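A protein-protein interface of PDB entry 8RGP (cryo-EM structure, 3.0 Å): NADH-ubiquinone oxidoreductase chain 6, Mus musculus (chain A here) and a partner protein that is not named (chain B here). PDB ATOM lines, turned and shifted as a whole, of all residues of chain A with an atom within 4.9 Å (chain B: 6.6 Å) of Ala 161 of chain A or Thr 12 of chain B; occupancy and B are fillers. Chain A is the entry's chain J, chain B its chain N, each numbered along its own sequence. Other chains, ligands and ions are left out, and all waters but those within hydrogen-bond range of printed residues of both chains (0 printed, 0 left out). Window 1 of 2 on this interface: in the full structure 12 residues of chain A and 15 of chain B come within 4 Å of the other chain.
The side-chain hydroxyl (OG1) of Thr 12 of chain B lies within hydrogen-bond range of the indole nitrogen (NE1) of Trp 157 of chain A.
CH2 of Trp 157 of chain A touches CD1 of Ile 8 of chain B, 3.6 Å away. Trp 157 of chain A touches Phe 11 of chain B (CZ2 to CD2, 3.5 Å). CD2 of Leu 15 of chain B touches CD1 of Trp 157 of chain A, 3.97 Å away. Trp 157 of chain A touches Phe 35 of chain B. CE1 of Phe 35 of chain B touches CA of Ser 158 of chain A, at 3.6 Å. Ala 161 of chain A touches Thr 12 of chain B. CD1 of Ile 165 of chain A touches O of Leu 38 of chain B, 3.2 Å away. CD1 of Ile 165 of chain A touches CA of Ala 39 of chain B, 3.95 Å away.
Of the 9 printed residues of chain A, 4 touch a printed residue of chain B. Hydrophobic or aromatic side chains of chain A within 4 Å of the printed part of chain B: Trp 157, Ala 161 and Ile 165. Hydrophobic or aromatic side chains of chain B within 4 Å of the printed part of chain A: Ile 8, Phe 11, Leu 15 and Phe 35. Among the printed residues, 9 pairs touch across the chains.
Of the printed residues of chain B, Trp 157 of chain A touches Ile 8, Phe 11, Thr 12, Leu 15 and Phe 35. Phe 160 of chain A touches none of the printed residues of chain B. Ala 161 of chain A touches just one residue of chain B: Thr 12. Printed residues of chain A within 4 Å of Phe 11 of chain B: Trp 157 (3.5 Å). Trp 133 of chain B touches none of the printed residues of chain A. The nearest residue of chain B that does not touch Ala 161 of chain A is Ile 8 of chain B (4.1 Å). The nearest printed residue of chain A that does not touch Phe 11 of chain B is Ala 161 of chain A (7.7 Å).
The side-chain hydroxyl (OG1) of Thr 12 of chain B sits at hydrogen-bond distance from the backbone carbonyl oxygen (O) of Ile 8 of chain B.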
ATOM      1  N   TRP A 157      18.137 -23.714 -18.106  1.00  0.00           N
ATOM      2  CA  TRP A 157      19.511 -23.377 -18.436  1.00  0.00           C
ATOM      3  C   TRP A 157      19.585 -22.149 -19.322  1.00  0.00           C
ATOM      4  O   TRP A 157      20.543 -21.381 -19.218  1.00  0.00           O
ATOM      5  CB  TRP A 157      20.210 -24.546 -19.117  1.00  0.00           C
ATOM      6  CG  TRP A 157      21.641 -24.252 -19.370  1.00  0.00           C
ATOM      7  CD1 TRP A 157      22.202 -23.866 -20.546  1.00  0.00           C
ATOM      8  CD2 TRP A 157      22.699 -24.283 -18.412  1.00  0.00           C
ATOM      9  NE1 TRP A 157      23.547 -23.669 -20.385  1.00  0.00           N
ATOM     10  CE2 TRP A 157      23.877 -23.920 -19.081  1.00  0.00           C
ATOM     11  CE3 TRP A 157      22.763 -24.588 -17.052  1.00  0.00           C
ATOM     12  CZ2 TRP A 157      25.105 -23.853 -18.440  1.00  0.00           C
ATOM     13  CZ3 TRP A 157      23.981 -24.522 -16.418  1.00  0.00           C
ATOM     14  CH2 TRP A 157      25.136 -24.159 -17.110  1.00  0.00           C
ATOM     15  N   SER A 158      18.593 -21.945 -20.192  1.00  0.00           N
ATOM     16  CA  SER A 158      18.563 -20.731 -20.993  1.00  0.00           C
ATOM     17  C   SER A 158      18.447 -19.501 -20.114  1.00  0.00           C
ATOM     18  O   SER A 158      19.164 -18.521 -20.320  1.00  0.00           O
ATOM     19  CB  SER A 158      17.406 -20.780 -21.981  1.00  0.00           C
ATOM     20  OG  SER A 158      16.176 -20.679 -21.295  1.00  0.00           O
ATOM     21  N   LEU A 159      17.588 -19.553 -19.097  1.00  0.00           N
ATOM     22  CA  LEU A 159      17.437 -18.394 -18.217  1.00  0.00           C
ATOM     23  C   LEU A 159      18.678 -18.171 -17.351  1.00  0.00           C
ATOM     24  O   LEU A 159      19.111 -17.026 -17.156  1.00  0.00           O
ATOM     25  CB  LEU A 159      16.188 -18.563 -17.359  1.00  0.00           C
ATOM     26  CG  LEU A 159      14.889 -18.557 -18.167  1.00  0.00           C
ATOM     27  CD1 LEU A 159      13.731 -19.029 -17.324  1.00  0.00           C
ATOM     28  CD2 LEU A 159      14.609 -17.174 -18.720  1.00  0.00           C
ATOM     29  N   PHE A 160      19.278 -19.252 -16.849  1.00  0.00           N
ATOM     30  CA  PHE A 160      20.489 -19.152 -16.033  1.00  0.00           C
ATOM     31  C   PHE A 160      21.660 -18.582 -16.834  1.00  0.00           C
ATOM     32  O   PHE A 160      22.306 -17.590 -16.431  1.00  0.00           O
ATOM     33  CB  PHE A 160      20.810 -20.550 -15.506  1.00  0.00           C
ATOM     34  CG  PHE A 160      21.843 -20.590 -14.432  1.00  0.00           C
ATOM     35  CD1 PHE A 160      21.561 -20.129 -13.165  1.00  0.00           C
ATOM     36  CD2 PHE A 160      23.080 -21.148 -14.677  1.00  0.00           C
ATOM     37  CE1 PHE A 160      22.508 -20.190 -12.172  1.00  0.00           C
ATOM     38  CE2 PHE A 160      24.029 -21.212 -13.688  1.00  0.00           C
ATOM     39  CZ  PHE A 160      23.742 -20.735 -12.435  1.00  0.00           C
ATOM     40  N   ALA A 161      21.930 -19.189 -17.992  1.00  0.00           N
ATOM     41  CA  ALA A 161      22.964 -18.698 -18.885  1.00  0.00           C
ATOM     42  C   ALA A 161      22.662 -17.283 -19.342  1.00  0.00           C
ATOM     43  O   ALA A 161      23.582 -16.489 -19.525  1.00  0.00           O
ATOM     44  CB  ALA A 161      23.110 -19.629 -20.085  1.00  0.00           C
ATOM     45  N   GLY A 162      21.381 -16.938 -19.496  1.00  0.00           N
ATOM     46  CA  GLY A 162      21.025 -15.582 -19.862  1.00  0.00           C
ATOM     47  C   GLY A 162      21.364 -14.568 -18.796  1.00  0.00           C
ATOM     48  O   GLY A 162      21.761 -13.448 -19.119  1.00  0.00           O
ATOM     49  N   ILE A 163      21.210 -14.938 -17.521  1.00  0.00           N
ATOM     50  CA  ILE A 163      21.647 -14.059 -16.434  1.00  0.00           C
ATOM     51  C   ILE A 163      23.144 -13.800 -16.537  1.00  0.00           C
ATOM     52  O   ILE A 163      23.608 -12.647 -16.474  1.00  0.00           O
ATOM     53  CB  ILE A 163      21.289 -14.668 -15.067  1.00  0.00           C
ATOM     54  CG1 ILE A 163      19.780 -14.709 -14.870  1.00  0.00           C
ATOM     55  CG2 ILE A 163      21.940 -13.883 -13.947  1.00  0.00           C
ATOM     56  CD1 ILE A 163      19.367 -15.498 -13.665  1.00  0.00           C
ATOM     57  N   PHE A 164      23.917 -14.870 -16.732  1.00  0.00           N
ATOM     58  CA  PHE A 164      25.365 -14.693 -16.867  1.00  0.00           C
ATOM     59  C   PHE A 164      25.716 -13.869 -18.106  1.00  0.00           C
ATOM     60  O   PHE A 164      26.601 -13.000 -18.062  1.00  0.00           O
ATOM     61  CB  PHE A 164      26.055 -16.052 -16.896  1.00  0.00           C
ATOM     62  CG  PHE A 164      26.200 -16.675 -15.545  1.00  0.00           C
ATOM     63  CD1 PHE A 164      25.138 -17.328 -14.951  1.00  0.00           C
ATOM     64  CD2 PHE A 164      27.394 -16.593 -14.860  1.00  0.00           C
ATOM     65  CE1 PHE A 164      25.270 -17.891 -13.705  1.00  0.00           C
ATOM     66  CE2 PHE A 164      27.532 -17.162 -13.615  1.00  0.00           C
ATOM     67  CZ  PHE A 164      26.467 -17.809 -13.037  1.00  0.00           C
ATOM     68  N   ILE A 165      24.983 -14.094 -19.196  1.00  0.00           N
ATOM     69  CA  ILE A 165      25.218 -13.410 -20.462  1.00  0.00           C
ATOM     70  C   ILE A 165      24.970 -11.914 -20.323  1.00  0.00           C
ATOM     71  O   ILE A 165      25.779 -11.096 -20.768  1.00  0.00           O
ATOM     72  CB  ILE A 165      24.338 -14.041 -21.558  1.00  0.00           C
ATOM     73  CG1 ILE A 165      25.005 -15.293 -22.127  1.00  0.00           C
ATOM     74  CG2 ILE A 165      24.000 -13.052 -22.662  1.00  0.00           C
ATOM     75  CD1 ILE A 165      24.033 -16.293 -22.698  1.00  0.00           C
ATOM     76  N   ALA B   7      33.111 -20.510 -17.680  1.00  0.00           N
ATOM     77  CA  ALA B   7      32.653 -21.888 -17.781  1.00  0.00           C
ATOM     78  C   ALA B   7      31.221 -21.956 -18.282  1.00  0.00           C
ATOM     79  O   ALA B   7      30.907 -22.777 -19.148  1.00  0.00           O
ATOM     80  CB  ALA B   7      32.782 -22.583 -16.428  1.00  0.00           C
ATOM     81  N   ILE B   8      30.349 -21.081 -17.772  1.00  0.00           N
ATOM     82  CA  ILE B   8      28.943 -21.100 -18.180  1.00  0.00           C
ATOM     83  C   ILE B   8      28.807 -20.766 -19.663  1.00  0.00           C
ATOM     84  O   ILE B   8      28.131 -21.478 -20.420  1.00  0.00           O
ATOM     85  CB  ILE B   8      28.114 -20.135 -17.312  1.00  0.00           C
ATOM     86  CG1 ILE B   8      28.099 -20.590 -15.854  1.00  0.00           C
ATOM     87  CG2 ILE B   8      26.696 -20.045 -17.823  1.00  0.00           C
ATOM     88  CD1 ILE B   8      27.607 -21.988 -15.660  1.00  0.00           C
ATOM     89  N   ILE B   9      29.483 -19.703 -20.105  1.00  0.00           N
ATOM     90  CA  ILE B   9      29.365 -19.249 -21.485  1.00  0.00           C
ATOM     91  C   ILE B   9      29.966 -20.263 -22.448  1.00  0.00           C
ATOM     92  O   ILE B   9      29.353 -20.602 -23.466  1.00  0.00           O
ATOM     93  CB  ILE B   9      30.010 -17.859 -21.631  1.00  0.00           C
ATOM     94  CG1 ILE B   9      29.106 -16.798 -21.003  1.00  0.00           C
ATOM     95  CG2 ILE B   9      30.284 -17.531 -23.079  1.00  0.00           C
ATOM     96  CD1 ILE B   9      29.618 -15.396 -21.144  1.00  0.00           C
ATOM     97  N   TYR B  10      31.159 -20.781 -22.139  1.00  0.00           N
ATOM     98  CA  TYR B  10      31.777 -21.754 -23.032  1.00  0.00           C
ATOM     99  C   TYR B  10      31.023 -23.074 -23.044  1.00  0.00           C
ATOM    100  O   TYR B  10      30.935 -23.719 -24.097  1.00  0.00           O
ATOM    101  CB  TYR B  10      33.235 -21.975 -22.648  1.00  0.00           C
ATOM    102  CG  TYR B  10      34.160 -20.973 -23.280  1.00  0.00           C
ATOM    103  CD1 TYR B  10      34.276 -20.890 -24.659  1.00  0.00           C
ATOM    104  CD2 TYR B  10      34.916 -20.111 -22.505  1.00  0.00           C
ATOM    105  CE1 TYR B  10      35.118 -19.978 -25.248  1.00  0.00           C
ATOM    106  CE2 TYR B  10      35.762 -19.190 -23.085  1.00  0.00           C
ATOM    107  CZ  TYR B  10      35.858 -19.129 -24.457  1.00  0.00           C
ATOM    108  OH  TYR B  10      36.702 -18.216 -25.041  1.00  0.00           O
ATOM    109  N   PHE B  11      30.453 -23.486 -21.909  1.00  0.00           N
ATOM    110  CA  PHE B  11      29.650 -24.698 -21.909  1.00  0.00           C
ATOM    111  C   PHE B  11      28.386 -24.519 -22.729  1.00  0.00           C
ATOM    112  O   PHE B  11      27.950 -25.454 -23.400  1.00  0.00           O
ATOM    113  CB  PHE B  11      29.299 -25.116 -20.485  1.00  0.00           C
ATOM    114  CG  PHE B  11      28.448 -26.346 -20.421  1.00  0.00           C
ATOM    115  CD1 PHE B  11      28.991 -27.587 -20.693  1.00  0.00           C
ATOM    116  CD2 PHE B  11      27.107 -26.263 -20.100  1.00  0.00           C
ATOM    117  CE1 PHE B  11      28.210 -28.725 -20.643  1.00  0.00           C
ATOM    118  CE2 PHE B  11      26.322 -27.396 -20.049  1.00  0.00           C
ATOM    119  CZ  PHE B  11      26.874 -28.628 -20.320  1.00  0.00           C
ATOM    120  N   THR B  12      27.782 -23.332 -22.698  1.00  0.00           N
ATOM    121  CA  THR B  12      26.587 -23.111 -23.508  1.00  0.00           C
ATOM    122  C   THR B  12      26.930 -23.035 -24.994  1.00  0.00           C
ATOM    123  O   THR B  12      26.152 -23.501 -25.840  1.00  0.00           O
ATOM    124  CB  THR B  12      25.876 -21.846 -23.044  1.00  0.00           C
ATOM    125  OG1 THR B  12      25.917 -21.777 -21.615  1.00  0.00           O
ATOM    126  CG2 THR B  12      24.430 -21.862 -23.495  1.00  0.00           C
ATOM    127  N   ILE B  13      28.093 -22.460 -25.323  1.00  0.00           N
ATOM    128  CA  ILE B  13      28.591 -22.468 -26.700  1.00  0.00           C
ATOM    129  C   ILE B  13      28.765 -23.898 -27.190  1.00  0.00           C
ATOM    130  O   ILE B  13      28.388 -24.234 -28.318  1.00  0.00           O
ATOM    131  CB  ILE B  13      29.910 -21.675 -26.802  1.00  0.00           C
ATOM    132  CG1 ILE B  13      29.658 -20.173 -26.716  1.00  0.00           C
ATOM    133  CG2 ILE B  13      30.641 -21.986 -28.094  1.00  0.00           C
ATOM    134  CD1 ILE B  13      30.910 -19.334 -26.834  1.00  0.00           C
ATOM    135  N   PHE B  14      29.330 -24.764 -26.349  1.00  0.00           N
ATOM    136  CA  PHE B  14      29.434 -26.176 -26.707  1.00  0.00           C
ATOM    137  C   PHE B  14      28.061 -26.837 -26.791  1.00  0.00           C
ATOM    138  O   PHE B  14      27.811 -27.647 -27.687  1.00  0.00           O
ATOM    139  CB  PHE B  14      30.317 -26.907 -25.698  1.00  0.00           C
ATOM    140  CG  PHE B  14      30.428 -28.382 -25.946  1.00  0.00           C
ATOM    141  CD1 PHE B  14      31.264 -28.867 -26.935  1.00  0.00           C
ATOM    142  CD2 PHE B  14      29.707 -29.285 -25.184  1.00  0.00           C
ATOM    143  CE1 PHE B  14      31.372 -30.221 -27.164  1.00  0.00           C
ATOM    144  CE2 PHE B  14      29.809 -30.640 -25.412  1.00  0.00           C
ATOM    145  CZ  PHE B  14      30.644 -31.107 -26.401  1.00  0.00           C
ATOM    146  N   LEU B  15      27.159 -26.488 -25.879  1.00  0.00           N
ATOM    147  CA  LEU B  15      25.909 -27.211 -25.704  1.00  0.00           C
ATOM    148  C   LEU B  15      24.913 -26.933 -26.814  1.00  0.00           C
ATOM    149  O   LEU B  15      24.084 -27.798 -27.117  1.00  0.00           O
ATOM    150  CB  LEU B  15      25.299 -26.844 -24.352  1.00  0.00           C
ATOM    151  CG  LEU B  15      24.077 -27.625 -23.874  1.00  0.00           C
ATOM    152  CD1 LEU B  15      24.446 -29.071 -23.613  1.00  0.00           C
ATOM    153  CD2 LEU B  15      23.489 -26.983 -22.633  1.00  0.00           C
ATOM    154  N   GLY B  16      24.964 -25.745 -27.412  1.00  0.00           N
ATOM    155  CA  GLY B  16      24.050 -25.383 -28.473  1.00  0.00           C
ATOM    156  C   GLY B  16      24.052 -26.322 -29.669  1.00  0.00           C
ATOM    157  O   GLY B  16      23.056 -27.002 -29.959  1.00  0.00           O
ATOM    158  N   PRO B  17      25.173 -26.363 -30.395  1.00  0.00           N
ATOM    159  CA  PRO B  17      25.291 -27.305 -31.515  1.00  0.00           C
ATOM    160  C   PRO B  17      25.135 -28.760 -31.126  1.00  0.00           C
ATOM    161  O   PRO B  17      24.634 -29.541 -31.940  1.00  0.00           O
ATOM    162  CB  PRO B  17      26.696 -27.021 -32.051  1.00  0.00           C
ATOM    163  CG  PRO B  17      26.900 -25.601 -31.758  1.00  0.00           C
ATOM    164  CD  PRO B  17      26.235 -25.347 -30.438  1.00  0.00           C
ATOM    165  N   GLY B  32      18.677 -25.216 -29.659  1.00  0.00           N
ATOM    166  CA  GLY B  32      20.125 -25.326 -29.755  1.00  0.00           C
ATOM    167  C   GLY B  32      20.748 -24.173 -30.519  1.00  0.00           C
ATOM    168  O   GLY B  32      21.797 -23.646 -30.127  1.00  0.00           O
ATOM    169  N   PHE B  35      20.672 -21.271 -28.222  1.00  0.00           N
ATOM    170  CA  PHE B  35      21.752 -21.433 -27.256  1.00  0.00           C
ATOM    171  C   PHE B  35      23.072 -20.955 -27.832  1.00  0.00           C
ATOM    172  O   PHE B  35      23.804 -20.198 -27.187  1.00  0.00           O
ATOM    173  CB  PHE B  35      21.867 -22.899 -26.850  1.00  0.00           C
ATOM    174  CG  PHE B  35      21.068 -23.263 -25.647  1.00  0.00           C
ATOM    175  CD1 PHE B  35      20.895 -22.362 -24.622  1.00  0.00           C
ATOM    176  CD2 PHE B  35      20.500 -24.515 -25.537  1.00  0.00           C
ATOM    177  CE1 PHE B  35      20.166 -22.700 -23.513  1.00  0.00           C
ATOM    178  CE2 PHE B  35      19.768 -24.855 -24.429  1.00  0.00           C
ATOM    179  CZ  PHE B  35      19.600 -23.948 -23.416  1.00  0.00           C
ATOM    180  N   SER B  36      23.374 -21.374 -29.063  1.00  0.00           N
ATOM    181  CA  SER B  36      24.641 -21.012 -29.690  1.00  0.00           C
ATOM    182  C   SER B  36      24.754 -19.505 -29.884  1.00  0.00           C
ATOM    183  O   SER B  36      25.777 -18.899 -29.541  1.00  0.00           O
ATOM    184  CB  SER B  36      24.785 -21.742 -31.025  1.00  0.00           C
ATOM    185  OG  SER B  36      26.112 -21.661 -31.505  1.00  0.00           O
ATOM    186  N   LEU B  38      22.994 -16.919 -28.370  1.00  0.00           N
ATOM    187  CA  LEU B  38      23.004 -16.140 -27.142  1.00  0.00           C
ATOM    188  C   LEU B  38      24.271 -16.376 -26.345  1.00  0.00           C
ATOM    189  O   LEU B  38      24.775 -15.450 -25.707  1.00  0.00           O
ATOM    190  CB  LEU B  38      21.774 -16.465 -26.301  1.00  0.00           C
ATOM    191  CG  LEU B  38      20.445 -16.167 -26.995  1.00  0.00           C
ATOM    192  CD1 LEU B  38      19.289 -16.444 -26.066  1.00  0.00           C
ATOM    193  CD2 LEU B  38      20.397 -14.744 -27.511  1.00  0.00           C
ATOM    194  N   ALA B  39      24.824 -17.588 -26.401  1.00  0.00           N
ATOM    195  CA  ALA B  39      26.070 -17.853 -25.707  1.00  0.00           C
ATOM    196  C   ALA B  39      27.253 -17.179 -26.382  1.00  0.00           C
ATOM    197  O   ALA B  39      28.172 -16.724 -25.694  1.00  0.00           O
ATOM    198  CB  ALA B  39      26.297 -19.354 -25.628  1.00  0.00           C
ATOM    199  N   ILE B  40      27.265 -17.103 -27.715  1.00  0.00           N
ATOM    200  CA  ILE B  40      28.453 -16.569 -28.366  1.00  0.00           C
ATOM    201  C   ILE B  40      28.462 -15.048 -28.402  1.00  0.00           C
ATOM    202  O   ILE B  40      29.524 -14.461 -28.638  1.00  0.00           O
ATOM    203  CB  ILE B  40      28.615 -17.137 -29.787  1.00  0.00           C
ATOM    204  CG1 ILE B  40      30.102 -17.196 -30.161  1.00  0.00           C
ATOM    205  CG2 ILE B  40      27.818 -16.328 -30.794  1.00  0.00           C
ATOM    206  CD1 ILE B  40      30.384 -17.387 -31.621  1.00  0.00           C
ATOM    207  N   TRP B 133      32.984 -23.267 -35.437  1.00  0.00           N
ATOM    208  CA  TRP B 133      32.005 -23.947 -34.605  1.00  0.00           C
ATOM    209  C   TRP B 133      30.577 -23.512 -34.908  1.00  0.00           C
ATOM    210  O   TRP B 133      29.659 -24.329 -34.782  1.00  0.00           O
ATOM    211  CB  TRP B 133      32.343 -23.708 -33.132  1.00  0.00           C
ATOM    212  CG  TRP B 133      31.489 -24.450 -32.160  1.00  0.00           C
ATOM    213  CD1 TRP B 133      30.590 -23.915 -31.291  1.00  0.00           C
ATOM    214  CD2 TRP B 133      31.461 -25.864 -31.945  1.00  0.00           C
ATOM    215  NE1 TRP B 133      29.999 -24.905 -30.551  1.00  0.00           N
ATOM    216  CE2 TRP B 133      30.515 -26.112 -30.936  1.00  0.00           C
ATOM    217  CE3 TRP B 133      32.139 -26.944 -32.513  1.00  0.00           C
ATOM    218  CZ2 TRP B 133      30.230 -27.393 -30.482  1.00  0.00           C
ATOM    219  CZ3 TRP B 133      31.855 -28.214 -32.061  1.00  0.00           C
ATOM    220  CH2 TRP B 133      30.911 -28.429 -31.054  1.00  0.00           C
